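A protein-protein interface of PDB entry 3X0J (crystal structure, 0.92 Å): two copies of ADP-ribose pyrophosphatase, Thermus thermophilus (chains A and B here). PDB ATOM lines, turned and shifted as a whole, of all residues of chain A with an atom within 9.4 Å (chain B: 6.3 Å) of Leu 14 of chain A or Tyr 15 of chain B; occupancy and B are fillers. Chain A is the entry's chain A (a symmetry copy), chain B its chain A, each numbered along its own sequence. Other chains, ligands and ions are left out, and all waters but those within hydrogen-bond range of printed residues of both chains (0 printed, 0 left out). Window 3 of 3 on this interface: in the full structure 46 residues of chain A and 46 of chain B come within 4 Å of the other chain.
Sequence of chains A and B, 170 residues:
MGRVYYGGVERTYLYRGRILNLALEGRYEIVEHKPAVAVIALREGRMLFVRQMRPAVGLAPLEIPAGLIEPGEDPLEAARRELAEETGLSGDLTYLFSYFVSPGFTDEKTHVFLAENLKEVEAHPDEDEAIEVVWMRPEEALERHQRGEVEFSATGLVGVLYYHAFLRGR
Leu 14 of chain A touches Tyr 15 of chain B. CE1 of Tyr 15 of chain A touches CD1 of Leu 14 of chain B (3.5 Å). Tyr 15 of chain A touches Leu 22 of chain B. Leu 20 of chain A touches Leu 22 of chain B (CD1 to CD1, 3.97 Å). Leu 22 of chain A touches Tyr 15 of chain B (CD2 to CD2, 3.6 Å). Leu 22 of chain A touches Leu 20 of chain B (CD1 to CD1, 3.97 Å). Leu 24 of chain A touches Tyr 15 of chain B. Gly 17 of chain B touches Glu 29 of chain A.
Printed residues of chain A that touch a printed residue of chain B: Leu 14, Tyr 15, Leu 20, Leu 22, Leu 24 and Glu 29. Hydrophobic or aromatic side chains of chain A within 4 Å of the printed part of chain B: Leu 14, Tyr 15, Leu 20, Leu 22 and Leu 24. Along chain A the printed residues that touch a printed residue of chain B span positions 14 to 29. Printed residues of chain B that touch a printed residue of chain A: Leu 14, Tyr 15, Gly 17, Arg 18, Leu 20 and Leu 22. Among the printed residues, no Asp or Glu carboxylate lies within 4 Å of a Lys or Arg side-chain nitrogen of the other chain.
Leu 14 of chain A touches one residue of chain B. Tyr 15 of chain B touches just these residues of chain A: Leu 14, Leu 22, Leu 24 and Glu 29. Of the printed residues of chain B, Leu 22 of chain A touches Tyr 15 (3.6 Å) and Leu 20 (3.97 Å). Printed residues of chain A within 4 Å of Arg 18 of chain B: Glu 29 (2.7 Å). Printed residues of chain B within 4 Å of Leu 20 of chain A: Leu 22 (3.97 Å). Of the printed residues of chain A, Gly 17 of chain B touches Glu 29 (3.2 Å). Val 31 of chain A touches none of the printed residues of chain B. The nearest printed residue of chain B that does not touch Leu 14 of chain A is Leu 22 of chain B (6.3 Å). The nearest printed residue of chain A that does not touch Tyr 15 of chain B is Tyr 15 of chain A (6.8 Å). The nearest printed residue of chain B that does not touch Glu 29 of chain A is Leu 20 of chain B (4.01 Å).
The backbone NH of Leu 14 of chain B sits at hydrogen-bond distance from the backbone carbonyl oxygen of Leu 22 of chain B (2.9 Å). O of Tyr 15 of chain B lies within hydrogen-bond range of N of Leu 22 of chain B. The side-chain amide oxygen of Asn 21 of chain B sits at hydrogen-bond distance from the backbone NH of Gly 17 of chain B, 3.2 Å away. N of Leu 24 of chain A is in hydrogen-bond range of O of Thr 12 of chain A. The backbone NH of Leu 14 of chain A is in hydrogen-bond range of the backbone carbonyl oxygen of Leu 22 of chain A (2.9 Å). N of Leu 22 of chain A sits at hydrogen-bond distance from O of Tyr 15 of chain A, 2.8 Å away.
OH of Tyr 15 of chain B is in hydrogen-bond range of OE2 of Glu 29 of chain A, at 2.6 Å. The backbone NH (N) of Arg 18 of chain B is in hydrogen-bond range of the side-chain carboxylate (OE2) of Glu 29 of chain A, 2.7 Å away.
Leu 14 of chain A touches Tyr 15 of chain B, and with the chains exchanged Tyr 15 of chain A touches Leu 14 of chain B. Tyr 15 of chain A touches Leu 22 of chain B, and with the chains exchanged Leu 22 of chain A touches Tyr 15 of chain B. Leu 20 of chain A touches Leu 22 of chain B, and with the chains exchanged Leu 22 of chain A touches Leu 20 of chain B. Positions printed for both chains: 12, 13, 14, 15, 16, 17, 20, 21, 22 and 23.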
ATOM      1  N   ARG A  11     -16.541  -9.712  16.100  1.00  0.00           N
ATOM      2  CA  ARG A  11     -16.312  -9.884  14.682  1.00  0.00           C
ATOM      3  C   ARG A  11     -17.463 -10.681  14.056  1.00  0.00           C
ATOM      4  O   ARG A  11     -17.747 -11.797  14.438  1.00  0.00           O
ATOM      5  CB  ARG A  11     -15.009 -10.613  14.280  1.00  0.00           C
ATOM      6  CG  ARG A  11     -13.839  -9.710  14.053  1.00  0.00           C
ATOM      7  CD  ARG A  11     -12.555 -10.462  13.665  1.00  0.00           C
ATOM      8  NE  ARG A  11     -11.515  -9.490  14.000  1.00  0.00           N
ATOM      9  CZ  ARG A  11     -10.257  -9.650  13.733  1.00  0.00           C
ATOM     10  NH1 ARG A  11      -9.945 -10.784  13.116  1.00  0.00           N
ATOM     11  NH2 ARG A  11      -9.332  -8.734  14.051  1.00  0.00           N
ATOM     12  N   THR A  12     -18.036 -10.009  13.055  1.00  0.00           N
ATOM     13  CA  THR A  12     -19.121 -10.530  12.225  1.00  0.00           C
ATOM     14  C   THR A  12     -18.602 -10.929  10.847  1.00  0.00           C
ATOM     15  O   THR A  12     -18.012 -10.022  10.188  1.00  0.00           O
ATOM     16  CB  THR A  12     -20.200  -9.465  12.037  1.00  0.00           C
ATOM     17  OG1 THR A  12     -20.702  -9.055  13.325  1.00  0.00           O
ATOM     18  CG2 THR A  12     -21.410  -9.993  11.268  1.00  0.00           C
ATOM     19  N   TYR A  13     -18.784 -12.163  10.446  1.00  0.00           N
ATOM     20  CA  TYR A  13     -18.226 -12.626   9.210  1.00  0.00           C
ATOM     21  C   TYR A  13     -19.177 -12.355   8.056  1.00  0.00           C
ATOM     22  O   TYR A  13     -20.353 -12.750   8.137  1.00  0.00           O
ATOM     23  CB  TYR A  13     -17.782 -14.100   9.355  1.00  0.00           C
ATOM     24  CG  TYR A  13     -16.581 -14.111  10.309  1.00  0.00           C
ATOM     25  CD1 TYR A  13     -16.691 -14.152  11.674  1.00  0.00           C
ATOM     26  CD2 TYR A  13     -15.317 -13.997   9.720  1.00  0.00           C
ATOM     27  CE1 TYR A  13     -15.616 -14.131  12.541  1.00  0.00           C
ATOM     28  CE2 TYR A  13     -14.226 -13.976  10.556  1.00  0.00           C
ATOM     29  CZ  TYR A  13     -14.365 -14.033  11.914  1.00  0.00           C
ATOM     30  OH  TYR A  13     -13.295 -14.036  12.775  1.00  0.00           O
ATOM     31  N   LEU A  14     -18.725 -11.683   7.012  1.00  0.00           N
ATOM     32  CA  LEU A  14     -19.428 -11.552   5.755  1.00  0.00           C
ATOM     33  C   LEU A  14     -19.059 -12.701   4.783  1.00  0.00           C
ATOM     34  O   LEU A  14     -19.890 -13.002   3.946  1.00  0.00           O
ATOM     35  CB  LEU A  14     -19.171 -10.235   5.064  1.00  0.00           C
ATOM     36  CG  LEU A  14     -19.440  -8.985   5.870  1.00  0.00           C
ATOM     37  CD1 LEU A  14     -19.235  -7.730   5.046  1.00  0.00           C
ATOM     38  CD2 LEU A  14     -20.889  -9.067   6.348  1.00  0.00           C
ATOM     39  N   TYR A  15     -17.831 -13.215   4.871  1.00  0.00           N
ATOM     40  CA  TYR A  15     -17.383 -14.187   3.861  1.00  0.00           C
ATOM     41  C   TYR A  15     -16.281 -15.050   4.464  1.00  0.00           C
ATOM     42  O   TYR A  15     -15.376 -14.455   5.032  1.00  0.00           O
ATOM     43  CB  TYR A  15     -16.867 -13.486   2.602  1.00  0.00           C
ATOM     44  CG  TYR A  15     -16.207 -14.392   1.629  1.00  0.00           C
ATOM     45  CD1 TYR A  15     -16.980 -15.165   0.763  1.00  0.00           C
ATOM     46  CD2 TYR A  15     -14.807 -14.479   1.564  1.00  0.00           C
ATOM     47  CE1 TYR A  15     -16.415 -16.008  -0.152  1.00  0.00           C
ATOM     48  CE2 TYR A  15     -14.256 -15.351   0.623  1.00  0.00           C
ATOM     49  CZ  TYR A  15     -15.018 -16.112  -0.238  1.00  0.00           C
ATOM     50  OH  TYR A  15     -14.459 -16.980  -1.157  1.00  0.00           O
ATOM     51  N   ARG A  16     -16.386 -16.334   4.390  1.00  0.00           N
ATOM     52  CA  ARG A  16     -15.413 -17.259   4.850  1.00  0.00           C
ATOM     53  C   ARG A  16     -14.858 -17.998   3.630  1.00  0.00           C
ATOM     54  O   ARG A  16     -15.667 -18.706   3.077  1.00  0.00           O
ATOM     55  CB  ARG A  16     -15.879 -18.321   5.859  1.00  0.00           C
ATOM     56  CG  ARG A  16     -16.050 -17.563   7.196  1.00  0.00           C
ATOM     57  CD  ARG A  16     -16.790 -18.481   8.122  1.00  0.00           C
ATOM     58  NE  ARG A  16     -16.778 -18.120   9.512  1.00  0.00           N
ATOM     59  CZ  ARG A  16     -15.691 -17.982  10.272  1.00  0.00           C
ATOM     60  NH1 ARG A  16     -14.468 -18.172   9.762  1.00  0.00           N
ATOM     61  NH2 ARG A  16     -15.855 -17.648  11.557  1.00  0.00           N
ATOM     62  N   GLY A  17     -13.577 -17.820   3.324  1.00  0.00           N
ATOM     63  CA  GLY A  17     -13.036 -18.278   2.047  1.00  0.00           C
ATOM     64  C   GLY A  17     -11.867 -19.191   2.178  1.00  0.00           C
ATOM     65  O   GLY A  17     -11.630 -19.774   3.225  1.00  0.00           O
ATOM     66  N   LEU A  20      -8.807 -16.263   2.621  1.00  0.00           N
ATOM     67  CA  LEU A  20      -9.176 -15.108   3.406  1.00  0.00           C
ATOM     68  C   LEU A  20     -10.604 -15.278   3.943  1.00  0.00           C
ATOM     69  O   LEU A  20     -11.395 -15.997   3.346  1.00  0.00           O
ATOM     70  CB  LEU A  20      -8.987 -13.813   2.644  1.00  0.00           C
ATOM     71  CG  LEU A  20      -9.823 -13.603   1.387  1.00  0.00           C
ATOM     72  CD1 LEU A  20     -11.193 -13.038   1.664  1.00  0.00           C
ATOM     73  CD2 LEU A  20      -9.009 -12.722   0.425  1.00  0.00           C
ATOM     74  N   ASN A  21     -10.837 -14.508   5.002  1.00  0.00           N
ATOM     75  CA  ASN A  21     -12.203 -14.237   5.468  1.00  0.00           C
ATOM     76  C   ASN A  21     -12.390 -12.734   5.462  1.00  0.00           C
ATOM     77  O   ASN A  21     -11.420 -11.983   5.727  1.00  0.00           O
ATOM     78  CB  ASN A  21     -12.455 -14.737   6.891  1.00  0.00           C
ATOM     79  CG  ASN A  21     -12.130 -16.193   7.064  1.00  0.00           C
ATOM     80  OD1 ASN A  21     -12.456 -17.051   6.246  1.00  0.00           O
ATOM     81  ND2 ASN A  21     -11.488 -16.468   8.145  1.00  0.00           N
ATOM     82  N   LEU A  22     -13.605 -12.261   5.204  1.00  0.00           N
ATOM     83  CA  LEU A  22     -13.938 -10.883   5.395  1.00  0.00           C
ATOM     84  C   LEU A  22     -14.848 -10.722   6.604  1.00  0.00           C
ATOM     85  O   LEU A  22     -15.908 -11.391   6.689  1.00  0.00           O
ATOM     86  CB  LEU A  22     -14.631 -10.322   4.150  1.00  0.00           C
ATOM     87  CG  LEU A  22     -15.168  -8.892   4.265  1.00  0.00           C
ATOM     88  CD1 LEU A  22     -14.050  -7.840   4.431  1.00  0.00           C
ATOM     89  CD2 LEU A  22     -16.012  -8.579   3.043  1.00  0.00           C
ATOM     90  N   ALA A  23     -14.485  -9.847   7.506  1.00  0.00           N
ATOM     91  CA  ALA A  23     -15.240  -9.597   8.751  1.00  0.00           C
ATOM     92  C   ALA A  23     -15.442  -8.133   8.879  1.00  0.00           C
ATOM     93  O   ALA A  23     -14.684  -7.290   8.391  1.00  0.00           O
ATOM     94  CB  ALA A  23     -14.503 -10.195   9.915  1.00  0.00           C
ATOM     95  N   LEU A  24     -16.468  -7.738   9.624  1.00  0.00           N
ATOM     96  CA  LEU A  24     -16.648  -6.406  10.179  1.00  0.00           C
ATOM     97  C   LEU A  24     -16.436  -6.491  11.697  1.00  0.00           C
ATOM     98  O   LEU A  24     -16.907  -7.360  12.419  1.00  0.00           O
ATOM     99  CB  LEU A  24     -18.043  -5.813   9.900  1.00  0.00           C
ATOM    100  CG  LEU A  24     -18.410  -5.799   8.403  1.00  0.00           C
ATOM    101  CD1 LEU A  24     -19.888  -5.385   8.274  1.00  0.00           C
ATOM    102  CD2 LEU A  24     -17.503  -4.914   7.582  1.00  0.00           C
ATOM    103  N   GLU A  25     -15.690  -5.506  12.195  1.00  0.00           N
ATOM    104  CA  GLU A  25     -15.448  -5.352  13.601  1.00  0.00           C
ATOM    105  C   GLU A  25     -15.771  -3.913  13.901  1.00  0.00           C
ATOM    106  O   GLU A  25     -14.921  -3.019  13.690  1.00  0.00           O
ATOM    107  CB  GLU A  25     -13.993  -5.652  13.938  1.00  0.00           C
ATOM    108  CG  GLU A  25     -13.786  -6.000  15.403  1.00  0.00           C
ATOM    109  CD  GLU A  25     -12.297  -6.127  15.663  1.00  0.00           C
ATOM    110  OE1 GLU A  25     -11.541  -6.836  14.951  1.00  0.00           O
ATOM    111  OE2 GLU A  25     -11.708  -5.511  16.579  1.00  0.00           O
ATOM    112  N   GLY A  26     -17.027  -3.725  14.356  1.00  0.00           N
ATOM    113  CA  GLY A  26     -17.453  -2.325  14.525  1.00  0.00           C
ATOM    114  C   GLY A  26     -17.444  -1.702  13.117  1.00  0.00           C
ATOM    115  O   GLY A  26     -18.007  -2.302  12.180  1.00  0.00           O
ATOM    116  N   ARG A  27     -16.757  -0.540  13.084  1.00  0.00           N
ATOM    117  CA  ARG A  27     -16.717   0.137  11.794  1.00  0.00           C
ATOM    118  C   ARG A  27     -15.630  -0.343  10.831  1.00  0.00           C
ATOM    119  O   ARG A  27     -15.439   0.113   9.699  1.00  0.00           O
ATOM    120  CB  ARG A  27     -16.549   1.634  12.010  1.00  0.00           C
ATOM    121  N   TYR A  28     -14.874  -1.328  11.308  1.00  0.00           N
ATOM    122  CA  TYR A  28     -13.649  -1.726  10.613  1.00  0.00           C
ATOM    123  C   TYR A  28     -13.928  -2.940   9.747  1.00  0.00           C
ATOM    124  O   TYR A  28     -14.536  -3.908  10.198  1.00  0.00           O
ATOM    125  CB  TYR A  28     -12.517  -2.027  11.583  1.00  0.00           C
ATOM    126  CG  TYR A  28     -11.954  -0.774  12.214  1.00  0.00           C
ATOM    127  CD1 TYR A  28     -10.931  -0.031  11.676  1.00  0.00           C
ATOM    128  CD2 TYR A  28     -12.544  -0.443  13.400  1.00  0.00           C
ATOM    129  CE1 TYR A  28     -10.512   1.076  12.368  1.00  0.00           C
ATOM    130  CE2 TYR A  28     -12.149   0.685  14.090  1.00  0.00           C
ATOM    131  CZ  TYR A  28     -11.118   1.435  13.541  1.00  0.00           C
ATOM    132  OH  TYR A  28     -10.745   2.540  14.258  1.00  0.00           O
ATOM    133  N   GLU A  29     -13.431  -2.843   8.541  1.00  0.00           N
ATOM    134  CA  GLU A  29     -13.466  -3.936   7.574  1.00  0.00           C
ATOM    135  C   GLU A  29     -12.122  -4.691   7.731  1.00  0.00           C
ATOM    136  O   GLU A  29     -11.051  -4.091   7.609  1.00  0.00           O
ATOM    137  CB  GLU A  29     -13.648  -3.420   6.150  1.00  0.00           C
ATOM    138  CG  GLU A  29     -14.946  -2.622   5.947  1.00  0.00           C
ATOM    139  CD  GLU A  29     -14.932  -1.656   4.809  1.00  0.00           C
ATOM    140  OE1 GLU A  29     -13.981  -0.910   4.567  1.00  0.00           O
ATOM    141  OE2 GLU A  29     -15.950  -1.588   4.060  1.00  0.00           O
ATOM    142  N   ILE A  30     -12.210  -5.976   7.987  1.00  0.00           N
ATOM    143  CA  ILE A  30     -10.998  -6.739   8.308  1.00  0.00           C
ATOM    144  C   ILE A  30     -10.957  -7.954   7.415  1.00  0.00           C
ATOM    145  O   ILE A  30     -11.909  -8.716   7.307  1.00  0.00           O
ATOM    146  CB  ILE A  30     -10.986  -7.119   9.819  1.00  0.00           C
ATOM    147  CG1 ILE A  30     -10.932  -5.884  10.752  1.00  0.00           C
ATOM    148  CG2 ILE A  30      -9.867  -8.093  10.122  1.00  0.00           C
ATOM    149  CD1 ILE A  30     -11.049  -6.188  12.237  1.00  0.00           C
ATOM    150  N   VAL A  31      -9.807  -8.155   6.786  1.00  0.00           N
ATOM    151  CA  VAL A  31      -9.541  -9.350   6.008  1.00  0.00           C
ATOM    152  C   VAL A  31      -8.589 -10.235   6.784  1.00  0.00           C
ATOM    153  O   VAL A  31      -7.398  -9.886   6.980  1.00  0.00           O
ATOM    154  CB  VAL A  31      -9.024  -9.017   4.641  1.00  0.00           C
ATOM    155  CG1 VAL A  31      -8.659 -10.315   3.882  1.00  0.00           C
ATOM    156  CG2 VAL A  31     -10.072  -8.224   3.840  1.00  0.00           C
ATOM    157  N   GLU A  32      -9.073 -11.359   7.239  1.00  0.00           N
ATOM    158  CA  GLU A  32      -8.223 -12.374   7.883  1.00  0.00           C
ATOM    159  C   GLU A  32      -7.553 -13.160   6.776  1.00  0.00           C
ATOM    160  O   GLU A  32      -8.187 -13.515   5.800  1.00  0.00           O
ATOM    161  CB  GLU A  32      -9.050 -13.324   8.784  1.00  0.00           C
ATOM    162  CG  GLU A  32      -9.721 -12.609   9.957  1.00  0.00           C
ATOM    163  CD  GLU A  32     -10.636 -13.439  10.772  1.00  0.00           C
ATOM    164  OE1 GLU A  32     -10.842 -14.686  10.350  1.00  0.00           O
ATOM    165  OE2 GLU A  32     -11.175 -12.986  11.756  1.00  0.00           O
ATOM    166  N   THR B  12     -16.803 -10.650 -10.160  1.00  0.00           N
ATOM    167  CA  THR B  12     -18.075 -10.693  -9.440  1.00  0.00           C
ATOM    168  C   THR B  12     -17.916 -10.132  -8.030  1.00  0.00           C
ATOM    169  O   THR B  12     -17.040 -10.687  -7.303  1.00  0.00           O
ATOM    170  CB  THR B  12     -18.567 -12.135  -9.324  1.00  0.00           C
ATOM    171  OG1 THR B  12     -18.715 -12.700 -10.642  1.00  0.00           O
ATOM    172  CG2 THR B  12     -19.948 -12.227  -8.676  1.00  0.00           C
ATOM    173  N   TYR B  13     -18.670  -9.123  -7.672  1.00  0.00           N
ATOM    174  CA  TYR B  13     -18.493  -8.483  -6.402  1.00  0.00           C
ATOM    175  C   TYR B  13     -19.316  -9.179  -5.330  1.00  0.00           C
ATOM    176  O   TYR B  13     -20.531  -9.358  -5.522  1.00  0.00           O
ATOM    177  CB  TYR B  13     -18.753  -6.965  -6.539  1.00  0.00           C
ATOM    178  CG  TYR B  13     -17.609  -6.392  -7.384  1.00  0.00           C
ATOM    179  CD1 TYR B  13     -17.605  -6.377  -8.753  1.00  0.00           C
ATOM    180  CD2 TYR B  13     -16.487  -5.934  -6.683  1.00  0.00           C
ATOM    181  CE1 TYR B  13     -16.566  -5.891  -9.523  1.00  0.00           C
ATOM    182  CE2 TYR B  13     -15.436  -5.442  -7.420  1.00  0.00           C
ATOM    183  CZ  TYR B  13     -15.466  -5.425  -8.786  1.00  0.00           C
ATOM    184  OH  TYR B  13     -14.442  -4.921  -9.550  1.00  0.00           O
ATOM    185  N   LEU B  14     -18.702  -9.595  -4.237  1.00  0.00           N
ATOM    186  CA  LEU B  14     -19.377 -10.057  -3.044  1.00  0.00           C
ATOM    187  C   LEU B  14     -19.655  -8.887  -2.067  1.00  0.00           C
ATOM    188  O   LEU B  14     -20.602  -9.011  -1.313  1.00  0.00           O
ATOM    189  CB  LEU B  14     -18.614 -11.129  -2.305  1.00  0.00           C
ATOM    190  CG  LEU B  14     -18.217 -12.349  -3.105  1.00  0.00           C
ATOM    191  CD1 LEU B  14     -17.540 -13.392  -2.241  1.00  0.00           C
ATOM    192  CD2 LEU B  14     -19.498 -12.921  -3.711  1.00  0.00           C
ATOM    193  N   TYR B  15     -18.789  -7.870  -2.058  1.00  0.00           N
ATOM    194  CA  TYR B  15     -18.920  -6.823  -1.034  1.00  0.00           C
ATOM    195  C   TYR B  15     -18.280  -5.542  -1.556  1.00  0.00           C
ATOM    196  O   TYR B  15     -17.158  -5.651  -2.029  1.00  0.00           O
ATOM    197  CB  TYR B  15     -18.256  -7.240   0.280  1.00  0.00           C
ATOM    198  CG  TYR B  15     -18.165  -6.154   1.288  1.00  0.00           C
ATOM    199  CD1 TYR B  15     -19.277  -5.833   2.066  1.00  0.00           C
ATOM    200  CD2 TYR B  15     -16.968  -5.446   1.474  1.00  0.00           C
ATOM    201  CE1 TYR B  15     -19.237  -4.845   3.009  1.00  0.00           C
ATOM    202  CE2 TYR B  15     -16.956  -4.438   2.441  1.00  0.00           C
ATOM    203  CZ  TYR B  15     -18.052  -4.122   3.215  1.00  0.00           C
ATOM    204  OH  TYR B  15     -18.029  -3.115   4.161  1.00  0.00           O
ATOM    205  N   ARG B  16     -18.960  -4.447  -1.519  1.00  0.00           N
ATOM    206  CA  ARG B  16     -18.476  -3.172  -1.911  1.00  0.00           C
ATOM    207  C   ARG B  16     -18.424  -2.288  -0.662  1.00  0.00           C
ATOM    208  O   ARG B  16     -19.510  -2.034  -0.197  1.00  0.00           O
ATOM    209  CB  ARG B  16     -19.280  -2.414  -2.978  1.00  0.00           C
ATOM    210  CG  ARG B  16     -18.972  -3.139  -4.310  1.00  0.00           C
ATOM    211  CD  ARG B  16     -19.963  -2.637  -5.315  1.00  0.00           C
ATOM    212  NE  ARG B  16     -19.667  -2.923  -6.692  1.00  0.00           N
ATOM    213  CZ  ARG B  16     -18.573  -2.538  -7.350  1.00  0.00           C
ATOM    214  NH1 ARG B  16     -17.619  -1.827  -6.739  1.00  0.00           N
ATOM    215  NH2 ARG B  16     -18.455  -2.883  -8.637  1.00  0.00           N
ATOM    216  N   GLY B  17     -17.234  -1.873  -0.241  1.00  0.00           N
ATOM    217  CA  GLY B  17     -17.073  -1.247   1.069  1.00  0.00           C
ATOM    218  C   GLY B  17     -16.437   0.099   1.021  1.00  0.00           C
ATOM    219  O   GLY B  17     -16.398   0.748  -0.013  1.00  0.00           O
ATOM    220  N   ARG B  18     -15.965   0.431   2.217  1.00  0.00           N
ATOM    221  CA  ARG B  18     -15.421   1.802   2.425  1.00  0.00           C
ATOM    222  C   ARG B  18     -13.972   1.807   2.001  1.00  0.00           C
ATOM    223  O   ARG B  18     -13.532   2.698   1.276  1.00  0.00           O
ATOM    224  CB  ARG B  18     -15.543   2.298   3.850  1.00  0.00           C
ATOM    225  N   LEU B  20     -12.357  -1.119   0.910  1.00  0.00           N
ATOM    226  CA  LEU B  20     -12.094  -2.298   0.120  1.00  0.00           C
ATOM    227  C   LEU B  20     -13.390  -2.782  -0.543  1.00  0.00           C
ATOM    228  O   LEU B  20     -14.470  -2.511  -0.033  1.00  0.00           O
ATOM    229  CB  LEU B  20     -11.407  -3.384   0.923  1.00  0.00           C
ATOM    230  CG  LEU B  20     -12.164  -3.975   2.105  1.00  0.00           C
ATOM    231  CD1 LEU B  20     -13.100  -5.093   1.722  1.00  0.00           C
ATOM    232  CD2 LEU B  20     -11.128  -4.412   3.153  1.00  0.00           C
ATOM    233  N   ASN B  21     -13.156  -3.551  -1.603  1.00  0.00           N
ATOM    234  CA  ASN B  21     -14.205  -4.401  -2.181  1.00  0.00           C
ATOM    235  C   ASN B  21     -13.691  -5.825  -2.160  1.00  0.00           C
ATOM    236  O   ASN B  21     -12.468  -6.051  -2.322  1.00  0.00           O
ATOM    237  CB  ASN B  21     -14.530  -4.040  -3.630  1.00  0.00           C
ATOM    238  CG  ASN B  21     -14.884  -2.590  -3.805  1.00  0.00           C
ATOM    239  OD1 ASN B  21     -15.634  -1.991  -3.036  1.00  0.00           O
ATOM    240  ND2 ASN B  21     -14.345  -2.032  -4.831  1.00  0.00           N
ATOM    241  N   LEU B  22     -14.579  -6.803  -1.999  1.00  0.00           N
ATOM    242  CA  LEU B  22     -14.234  -8.178  -2.190  1.00  0.00           C
ATOM    243  C   LEU B  22     -14.863  -8.708  -3.470  1.00  0.00           C
ATOM    244  O   LEU B  22     -16.098  -8.589  -3.662  1.00  0.00           O
ATOM    245  CB  LEU B  22     -14.705  -9.018  -0.998  1.00  0.00           C
ATOM    246  CG  LEU B  22     -14.524 -10.533  -1.131  1.00  0.00           C
ATOM    247  CD1 LEU B  22     -13.042 -10.962  -1.175  1.00  0.00           C
ATOM    248  CD2 LEU B  22     -15.239 -11.219   0.019  1.00  0.00           C
ATOM    249  N   ALA B  23     -14.065  -9.304  -4.318  1.00  0.00           N
ATOM    250  CA  ALA B  23     -14.513  -9.843  -5.619  1.00  0.00           C
ATOM    251  C   ALA B  23     -14.019 -11.237  -5.733  1.00  0.00           C
ATOM    252  O   ALA B  23     -13.008 -11.655  -5.164  1.00  0.00           O
ATOM    253  CB  ALA B  23     -14.028  -8.951  -6.727  1.00  0.00           C
